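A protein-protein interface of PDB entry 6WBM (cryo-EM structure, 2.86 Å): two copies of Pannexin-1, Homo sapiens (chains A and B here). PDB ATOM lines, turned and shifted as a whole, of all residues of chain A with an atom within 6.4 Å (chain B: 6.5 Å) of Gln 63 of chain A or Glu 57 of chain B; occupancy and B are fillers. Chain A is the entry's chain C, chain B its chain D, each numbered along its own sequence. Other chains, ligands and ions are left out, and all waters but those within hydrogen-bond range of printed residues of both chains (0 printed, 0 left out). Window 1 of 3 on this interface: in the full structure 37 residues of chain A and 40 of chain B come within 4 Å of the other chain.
O of Gln 56 of chain B is in hydrogen-bond range of NE2 of Gln 63 of chain A (3.2 Å). The indole nitrogen (NE1) of Trp 85 of chain A sits at hydrogen-bond distance from the backbone carbonyl oxygen (O) of Ile 58 of chain B, at 3.0 Å.
O of Gln 63 of chain A is in hydrogen-bond range of N of Ile 268 of chain A, at 3.0 Å. The side-chain carboxylate of Glu 57 of chain B lies close to the backbone NH of Ile 3 of chain B (3.1 Å). NZ of Lys 107 of chain A is in hydrogen-bond range of O of Trp 85 of chain A (3.1 Å). The backbone carbonyl oxygen (O) of Ala 55 of chain B lies within hydrogen-bond range of the side-chain hydroxyl (OG) of Ser 59 of chain B (3.0 Å). O of Ile 64 of chain A sits at hydrogen-bond distance from OG1 of Thr 62 of chain A (2.8 Å).
Among the printed residues, merely in contact across the chains: Lys 107 of chain A with Ile 58 of chain B (3.2 Å), Gln 63 of chain A with Ile 60 of chain B (3.2 Å), Phe 54 of chain A with Glu 57 of chain B (3.3 Å), Tyr 111 of chain A with Ile 58 of chain B (3.4 Å), Tyr 111 of chain A with Ile 3 of chain B (3.4 Å), Trp 85 of chain A with Ile 60 of chain B (3.5 Å), Gln 63 of chain A with Glu 57 of chain B (3.6 Å), Ile 64 of chain A with Ile 60 of chain B (3.8 Å), Pro 110 of chain A with Ile 3 of chain B (3.9 Å), Gln 63 of chain A with Ser 59 of chain B (3.98 Å) and Ile 50 of chain A with Ile 3 of chain B (3.99 Å).
Printed residues of chain B within 4 Å of Ile 50 of chain A: Ile 3. Printed residues of chain B within 4 Å of Gln 63 of chain A: Gln 56, Glu 57, Ser 59 and Ile 60. Of the printed residues of chain B, Tyr 111 of chain A touches Ile 3 and Ile 58. Of the printed residues of chain A, Gln 56 of chain B touches Gln 63 (3.2 Å). Of chain A, only Phe 54 (3.3 Å) and Gln 63 (3.6 Å) come within 4 Å of Glu 57 of chain B. Of the printed residues of chain A, Ile 60 of chain B touches Gln 63, Ile 64 and Trp 85. The nearest printed residue of chain B that does not touch Gln 63 of chain A is Ile 58 of chain B (4.3 Å).
Of the 16 printed residues of chain A, 8 touch a printed residue of chain B. Hydrophobic or aromatic side chains of chain A that line the printed part of chain B: Ile 50, Phe 54, Ile 64, Trp 85, Pro 110 and Tyr 111. Printed residues of chain B that touch a printed residue of chain A: Ile 3, Gln 56, Glu 57, Ile 58, Ser 59 and Ile 60. Hydrophobic or aromatic side chains of chain B that line the printed part of chain A: Ile 3, Ile 58 and Ile 60. Among the printed residues, no Asp or Glu carboxylate lies within 4 Å of a Lys or Arg side-chain nitrogen of the other chain.
2 positions are printed for both chains.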
ATOM      1  N   ILE A  50     -37.900 -30.130  10.218  1.00  0.00           N
ATOM      2  CA  ILE A  50     -36.445 -30.085  10.116  1.00  0.00           C
ATOM      3  C   ILE A  50     -36.031 -29.848   8.674  1.00  0.00           C
ATOM      4  O   ILE A  50     -35.209 -28.975   8.378  1.00  0.00           O
ATOM      5  CB  ILE A  50     -35.827 -31.381  10.663  1.00  0.00           C
ATOM      6  CG1 ILE A  50     -35.793 -31.363  12.184  1.00  0.00           C
ATOM      7  CG2 ILE A  50     -34.430 -31.569  10.118  1.00  0.00           C
ATOM      8  CD1 ILE A  50     -35.230 -32.632  12.767  1.00  0.00           C
ATOM      9  N   PHE A  54     -34.304 -25.826   6.680  1.00  0.00           N
ATOM     10  CA  PHE A  54     -33.074 -25.659   5.920  1.00  0.00           C
ATOM     11  C   PHE A  54     -33.293 -25.854   4.430  1.00  0.00           C
ATOM     12  O   PHE A  54     -32.340 -26.149   3.702  1.00  0.00           O
ATOM     13  CB  PHE A  54     -32.008 -26.620   6.435  1.00  0.00           C
ATOM     14  CG  PHE A  54     -31.667 -26.410   7.869  1.00  0.00           C
ATOM     15  CD1 PHE A  54     -30.678 -25.519   8.230  1.00  0.00           C
ATOM     16  CD2 PHE A  54     -32.343 -27.089   8.859  1.00  0.00           C
ATOM     17  CE1 PHE A  54     -30.362 -25.322   9.549  1.00  0.00           C
ATOM     18  CE2 PHE A  54     -32.030 -26.894  10.178  1.00  0.00           C
ATOM     19  CZ  PHE A  54     -31.038 -26.012  10.522  1.00  0.00           C
ATOM     20  N   GLY A  61     -28.029 -18.936   3.726  1.00  0.00           N
ATOM     21  CA  GLY A  61     -26.627 -19.291   3.707  1.00  0.00           C
ATOM     22  C   GLY A  61     -26.174 -19.870   5.028  1.00  0.00           C
ATOM     23  O   GLY A  61     -26.741 -20.853   5.510  1.00  0.00           O
ATOM     24  N   THR A  62     -25.139 -19.274   5.613  1.00  0.00           N
ATOM     25  CA  THR A  62     -24.614 -19.732   6.886  1.00  0.00           C
ATOM     26  C   THR A  62     -25.693 -19.679   7.966  1.00  0.00           C
ATOM     27  O   THR A  62     -26.733 -19.034   7.821  1.00  0.00           O
ATOM     28  CB  THR A  62     -23.425 -18.873   7.311  1.00  0.00           C
ATOM     29  OG1 THR A  62     -23.842 -17.506   7.417  1.00  0.00           O
ATOM     30  CG2 THR A  62     -22.304 -18.974   6.291  1.00  0.00           C
ATOM     31  N   GLN A  63     -25.427 -20.377   9.067  1.00  0.00           N
ATOM     32  CA  GLN A  63     -26.292 -20.317  10.234  1.00  0.00           C
ATOM     33  C   GLN A  63     -25.879 -19.235  11.213  1.00  0.00           C
ATOM     34  O   GLN A  63     -26.571 -19.032  12.214  1.00  0.00           O
ATOM     35  CB  GLN A  63     -26.309 -21.663  10.960  1.00  0.00           C
ATOM     36  CG  GLN A  63     -26.724 -22.828  10.098  1.00  0.00           C
ATOM     37  CD  GLN A  63     -25.552 -23.476   9.405  1.00  0.00           C
ATOM     38  OE1 GLN A  63     -24.429 -22.980   9.467  1.00  0.00           O
ATOM     39  NE2 GLN A  63     -25.804 -24.594   8.739  1.00  0.00           N
ATOM     40  N   ILE A  64     -24.773 -18.544  10.954  1.00  0.00           N
ATOM     41  CA  ILE A  64     -24.253 -17.538  11.864  1.00  0.00           C
ATOM     42  C   ILE A  64     -23.454 -16.518  11.065  1.00  0.00           C
ATOM     43  O   ILE A  64     -22.895 -16.828  10.009  1.00  0.00           O
ATOM     44  CB  ILE A  64     -23.386 -18.175  12.969  1.00  0.00           C
ATOM     45  CG1 ILE A  64     -23.012 -17.144  14.029  1.00  0.00           C
ATOM     46  CG2 ILE A  64     -22.150 -18.803  12.371  1.00  0.00           C
ATOM     47  CD1 ILE A  64     -22.165 -17.700  15.135  1.00  0.00           C
ATOM     48  N   SER A  65     -23.424 -15.288  11.565  1.00  0.00           N
ATOM     49  CA  SER A  65     -22.598 -14.235  11.000  1.00  0.00           C
ATOM     50  C   SER A  65     -22.216 -13.298  12.130  1.00  0.00           C
ATOM     51  O   SER A  65     -23.016 -13.068  13.038  1.00  0.00           O
ATOM     52  CB  SER A  65     -23.328 -13.473   9.898  1.00  0.00           C
ATOM     53  OG  SER A  65     -23.963 -14.370   9.012  1.00  0.00           O
ATOM     54  N   TRP A  85     -19.246 -19.734  16.286  1.00  0.00           N
ATOM     55  CA  TRP A  85     -20.140 -20.871  16.108  1.00  0.00           C
ATOM     56  C   TRP A  85     -19.757 -22.018  17.031  1.00  0.00           C
ATOM     57  O   TRP A  85     -20.620 -22.648  17.650  1.00  0.00           O
ATOM     58  CB  TRP A  85     -20.113 -21.328  14.653  1.00  0.00           C
ATOM     59  CG  TRP A  85     -20.926 -22.540  14.392  1.00  0.00           C
ATOM     60  CD1 TRP A  85     -20.464 -23.777  14.081  1.00  0.00           C
ATOM     61  CD2 TRP A  85     -22.349 -22.632  14.401  1.00  0.00           C
ATOM     62  NE1 TRP A  85     -21.510 -24.641  13.898  1.00  0.00           N
ATOM     63  CE2 TRP A  85     -22.682 -23.960  14.090  1.00  0.00           C
ATOM     64  CE3 TRP A  85     -23.376 -21.721  14.644  1.00  0.00           C
ATOM     65  CZ2 TRP A  85     -23.994 -24.398  14.016  1.00  0.00           C
ATOM     66  CZ3 TRP A  85     -24.675 -22.158  14.571  1.00  0.00           C
ATOM     67  CH2 TRP A  85     -24.975 -23.483  14.259  1.00  0.00           C
ATOM     68  N   LYS A 107     -28.567 -23.611  18.490  1.00  0.00           N
ATOM     69  CA  LYS A 107     -27.640 -24.345  17.641  1.00  0.00           C
ATOM     70  C   LYS A 107     -28.129 -25.760  17.377  1.00  0.00           C
ATOM     71  O   LYS A 107     -28.029 -26.258  16.252  1.00  0.00           O
ATOM     72  CB  LYS A 107     -26.252 -24.373  18.271  1.00  0.00           C
ATOM     73  CG  LYS A 107     -25.215 -25.062  17.412  1.00  0.00           C
ATOM     74  CD  LYS A 107     -23.867 -25.087  18.092  1.00  0.00           C
ATOM     75  CE  LYS A 107     -22.804 -25.670  17.190  1.00  0.00           C
ATOM     76  NZ  LYS A 107     -21.474 -25.669  17.851  1.00  0.00           N
ATOM     77  N   PRO A 110     -32.281 -28.602  15.394  1.00  0.00           N
ATOM     78  CA  PRO A 110     -32.564 -29.780  14.559  1.00  0.00           C
ATOM     79  C   PRO A 110     -32.288 -31.086  15.270  1.00  0.00           C
ATOM     80  O   PRO A 110     -33.056 -32.044  15.123  1.00  0.00           O
ATOM     81  CB  PRO A 110     -31.637 -29.586  13.354  1.00  0.00           C
ATOM     82  CG  PRO A 110     -31.318 -28.154  13.345  1.00  0.00           C
ATOM     83  CD  PRO A 110     -31.268 -27.740  14.767  1.00  0.00           C
ATOM     84  N   TYR A 111     -31.204 -31.154  16.041  1.00  0.00           N
ATOM     85  CA  TYR A 111     -30.906 -32.380  16.768  1.00  0.00           C
ATOM     86  C   TYR A 111     -31.993 -32.689  17.781  1.00  0.00           C
ATOM     87  O   TYR A 111     -32.357 -33.852  17.972  1.00  0.00           O
ATOM     88  CB  TYR A 111     -29.554 -32.263  17.462  1.00  0.00           C
ATOM     89  CG  TYR A 111     -28.383 -32.425  16.533  1.00  0.00           C
ATOM     90  CD1 TYR A 111     -28.569 -32.548  15.168  1.00  0.00           C
ATOM     91  CD2 TYR A 111     -27.089 -32.457  17.024  1.00  0.00           C
ATOM     92  CE1 TYR A 111     -27.504 -32.695  14.319  1.00  0.00           C
ATOM     93  CE2 TYR A 111     -26.018 -32.604  16.182  1.00  0.00           C
ATOM     94  CZ  TYR A 111     -26.231 -32.724  14.830  1.00  0.00           C
ATOM     95  OH  TYR A 111     -25.162 -32.868  13.985  1.00  0.00           O
ATOM     96  N   LYS A 266     -24.864 -13.081  15.162  1.00  0.00           N
ATOM     97  CA  LYS A 266     -26.299 -13.317  15.142  1.00  0.00           C
ATOM     98  C   LYS A 266     -26.574 -14.679  14.536  1.00  0.00           C
ATOM     99  O   LYS A 266     -26.087 -14.986  13.446  1.00  0.00           O
ATOM    100  CB  LYS A 266     -27.047 -12.245  14.348  1.00  0.00           C
ATOM    101  CG  LYS A 266     -28.517 -12.576  14.156  1.00  0.00           C
ATOM    102  CD  LYS A 266     -29.295 -11.385  13.654  1.00  0.00           C
ATOM    103  CE  LYS A 266     -30.788 -11.588  13.819  1.00  0.00           C
ATOM    104  NZ  LYS A 266     -31.198 -11.633  15.246  1.00  0.00           N
ATOM    105  N   LEU A 267     -27.361 -15.483  15.240  1.00  0.00           N
ATOM    106  CA  LEU A 267     -27.719 -16.817  14.773  1.00  0.00           C
ATOM    107  C   LEU A 267     -28.858 -16.685  13.776  1.00  0.00           C
ATOM    108  O   LEU A 267     -30.020 -16.543  14.157  1.00  0.00           O
ATOM    109  CB  LEU A 267     -28.111 -17.705  15.945  1.00  0.00           C
ATOM    110  CG  LEU A 267     -26.935 -18.222  16.763  1.00  0.00           C
ATOM    111  CD1 LEU A 267     -27.423 -18.817  18.057  1.00  0.00           C
ATOM    112  CD2 LEU A 267     -26.176 -19.250  15.963  1.00  0.00           C
ATOM    113  N   ILE A 268     -28.524 -16.725  12.487  1.00  0.00           N
ATOM    114  CA  ILE A 268     -29.555 -16.717  11.467  1.00  0.00           C
ATOM    115  C   ILE A 268     -30.391 -17.986  11.592  1.00  0.00           C
ATOM    116  O   ILE A 268     -29.996 -18.967  12.233  1.00  0.00           O
ATOM    117  CB  ILE A 268     -28.938 -16.596  10.067  1.00  0.00           C
ATOM    118  CG1 ILE A 268     -27.740 -15.654  10.105  1.00  0.00           C
ATOM    119  CG2 ILE A 268     -29.951 -16.071   9.077  1.00  0.00           C
ATOM    120  CD1 ILE A 268     -28.101 -14.236  10.466  1.00  0.00           C
ATOM    121  N   ALA A 269     -31.574 -17.955  10.982  1.00  0.00           N
ATOM    122  CA  ALA A 269     -32.504 -19.077  10.953  1.00  0.00           C
ATOM    123  C   ALA A 269     -33.026 -19.439  12.333  1.00  0.00           C
ATOM    124  O   ALA A 269     -33.355 -20.599  12.584  1.00  0.00           O
ATOM    125  CB  ALA A 269     -31.881 -20.311  10.291  1.00  0.00           C
ATOM    126  N   PHE A 273     -36.846 -21.236  13.086  1.00  0.00           N
ATOM    127  CA  PHE A 273     -36.927 -22.275  14.102  1.00  0.00           C
ATOM    128  C   PHE A 273     -38.116 -22.051  15.015  1.00  0.00           C
ATOM    129  O   PHE A 273     -38.876 -22.982  15.287  1.00  0.00           O
ATOM    130  CB  PHE A 273     -35.639 -22.323  14.917  1.00  0.00           C
ATOM    131  CG  PHE A 273     -34.485 -22.926  14.188  1.00  0.00           C
ATOM    132  CD1 PHE A 273     -34.671 -23.567  12.981  1.00  0.00           C
ATOM    133  CD2 PHE A 273     -33.211 -22.854  14.712  1.00  0.00           C
ATOM    134  CE1 PHE A 273     -33.610 -24.119  12.312  1.00  0.00           C
ATOM    135  CE2 PHE A 273     -32.148 -23.406  14.047  1.00  0.00           C
ATOM    136  CZ  PHE A 273     -32.348 -24.038  12.846  1.00  0.00           C
ATOM    137  N   ALA B   2     -29.411 -34.188   4.212  1.00  0.00           N
ATOM    138  CA  ALA B   2     -30.343 -33.655   5.195  1.00  0.00           C
ATOM    139  C   ALA B   2     -30.441 -34.584   6.394  1.00  0.00           C
ATOM    140  O   ALA B   2     -30.228 -35.788   6.274  1.00  0.00           O
ATOM    141  CB  ALA B   2     -31.712 -33.450   4.575  1.00  0.00           C
ATOM    142  N   ILE B   3     -30.767 -34.010   7.552  1.00  0.00           N
ATOM    143  CA  ILE B   3     -30.885 -34.807   8.768  1.00  0.00           C
ATOM    144  C   ILE B   3     -31.997 -35.835   8.640  1.00  0.00           C
ATOM    145  O   ILE B   3     -31.830 -36.992   9.043  1.00  0.00           O
ATOM    146  CB  ILE B   3     -31.103 -33.887   9.981  1.00  0.00           C
ATOM    147  CG1 ILE B   3     -29.763 -33.480  10.584  1.00  0.00           C
ATOM    148  CG2 ILE B   3     -31.958 -34.565  11.030  1.00  0.00           C
ATOM    149  CD1 ILE B   3     -29.895 -32.676  11.844  1.00  0.00           C
ATOM    150  N   ALA B   4     -33.138 -35.447   8.071  1.00  0.00           N
ATOM    151  CA  ALA B   4     -34.272 -36.357   8.006  1.00  0.00           C
ATOM    152  C   ALA B   4     -33.979 -37.573   7.137  1.00  0.00           C
ATOM    153  O   ALA B   4     -34.490 -38.664   7.408  1.00  0.00           O
ATOM    154  CB  ALA B   4     -35.502 -35.616   7.496  1.00  0.00           C
ATOM    155  N   PHE B  54     -21.650 -34.147  10.929  1.00  0.00           N
ATOM    156  CA  PHE B  54     -21.273 -33.397   9.741  1.00  0.00           C
ATOM    157  C   PHE B  54     -22.469 -33.093   8.854  1.00  0.00           C
ATOM    158  O   PHE B  54     -22.299 -32.842   7.659  1.00  0.00           O
ATOM    159  CB  PHE B  54     -20.208 -34.157   8.960  1.00  0.00           C
ATOM    160  CG  PHE B  54     -18.961 -34.395   9.738  1.00  0.00           C
ATOM    161  CD1 PHE B  54     -17.943 -33.464   9.730  1.00  0.00           C
ATOM    162  CD2 PHE B  54     -18.811 -35.538  10.492  1.00  0.00           C
ATOM    163  CE1 PHE B  54     -16.795 -33.679  10.447  1.00  0.00           C
ATOM    164  CE2 PHE B  54     -17.665 -35.756  11.209  1.00  0.00           C
ATOM    165  CZ  PHE B  54     -16.656 -34.826  11.186  1.00  0.00           C
ATOM    166  N   ALA B  55     -23.673 -33.129   9.411  1.00  0.00           N
ATOM    167  CA  ALA B  55     -24.842 -32.711   8.657  1.00  0.00           C
ATOM    168  C   ALA B  55     -24.680 -31.263   8.225  1.00  0.00           C
ATOM    169  O   ALA B  55     -24.109 -30.443   8.947  1.00  0.00           O
ATOM    170  CB  ALA B  55     -26.105 -32.876   9.498  1.00  0.00           C
ATOM    171  N   GLN B  56     -25.181 -30.951   7.030  1.00  0.00           N
ATOM    172  CA  GLN B  56     -25.045 -29.602   6.501  1.00  0.00           C
ATOM    173  C   GLN B  56     -25.752 -28.570   7.364  1.00  0.00           C
ATOM    174  O   GLN B  56     -25.543 -27.369   7.172  1.00  0.00           O
ATOM    175  CB  GLN B  56     -25.585 -29.543   5.073  1.00  0.00           C
ATOM    176  CG  GLN B  56     -25.373 -28.205   4.403  1.00  0.00           C
ATOM    177  CD  GLN B  56     -23.905 -27.884   4.219  1.00  0.00           C
ATOM    178  OE1 GLN B  56     -23.176 -28.617   3.550  1.00  0.00           O
ATOM    179  NE2 GLN B  56     -23.461 -26.785   4.816  1.00  0.00           N
ATOM    180  N   GLU B  57     -26.574 -29.011   8.310  1.00  0.00           N
ATOM    181  CA  GLU B  57     -27.354 -28.126   9.153  1.00  0.00           C
ATOM    182  C   GLU B  57     -26.657 -27.773  10.457  1.00  0.00           C
ATOM    183  O   GLU B  57     -27.155 -26.919  11.194  1.00  0.00           O
ATOM    184  CB  GLU B  57     -28.708 -28.773   9.449  1.00  0.00           C
ATOM    185  CG  GLU B  57     -29.569 -28.900   8.210  1.00  0.00           C
ATOM    186  CD  GLU B  57     -29.692 -30.322   7.715  1.00  0.00           C
ATOM    187  OE1 GLU B  57     -29.733 -30.528   6.484  1.00  0.00           O
ATOM    188  OE2 GLU B  57     -29.756 -31.235   8.556  1.00  0.00           O
ATOM    189  N   ILE B  58     -25.528 -28.406  10.756  1.00  0.00           N
ATOM    190  CA  ILE B  58     -24.778 -28.114  11.969  1.00  0.00           C
ATOM    191  C   ILE B  58     -23.388 -27.627  11.591  1.00  0.00           C
ATOM    192  O   ILE B  58     -22.871 -26.667  12.172  1.00  0.00           O
ATOM    193  CB  ILE B  58     -24.706 -29.346  12.884  1.00  0.00           C
ATOM    194  CG1 ILE B  58     -26.036 -29.538  13.600  1.00  0.00           C
ATOM    195  CG2 ILE B  58     -23.599 -29.192  13.896  1.00  0.00           C
ATOM    196  CD1 ILE B  58     -26.357 -28.426  14.558  1.00  0.00           C
ATOM    197  N   SER B  59     -22.776 -28.285  10.613  1.00  0.00           N
ATOM    198  CA  SER B  59     -21.430 -27.926  10.196  1.00  0.00           C
ATOM    199  C   SER B  59     -21.425 -26.541   9.566  1.00  0.00           C
ATOM    200  O   SER B  59     -22.189 -26.266   8.636  1.00  0.00           O
ATOM    201  CB  SER B  59     -20.890 -28.958   9.212  1.00  0.00           C
ATOM    202  OG  SER B  59     -21.657 -28.966   8.023  1.00  0.00           O
ATOM    203  N   ILE B  60     -20.559 -25.669  10.075  1.00  0.00           N
ATOM    204  CA  ILE B  60     -20.473 -24.315   9.545  1.00  0.00           C
ATOM    205  C   ILE B  60     -19.598 -24.272   8.302  1.00  0.00           C
ATOM    206  O   ILE B  60     -19.722 -23.356   7.482  1.00  0.00           O
ATOM    207  CB  ILE B  60     -19.952 -23.359  10.628  1.00  0.00           C
ATOM    208  CG1 ILE B  60     -20.127 -21.905  10.198  1.00  0.00           C
ATOM    209  CG2 ILE B  60     -18.494 -23.639  10.922  1.00  0.00           C
ATOM    210  CD1 ILE B  60     -21.528 -21.566   9.773  1.00  0.00           C
ATOM    211  N   GLY B  61     -18.721 -25.252   8.126  1.00  0.00           N
ATOM    212  CA  GLY B  61     -17.742 -25.189   7.062  1.00  0.00           C
ATOM    213  C   GLY B  61     -16.541 -26.061   7.347  1.00  0.00           C
ATOM    214  O   GLY B  61     -16.681 -27.265   7.577  1.00  0.00           O
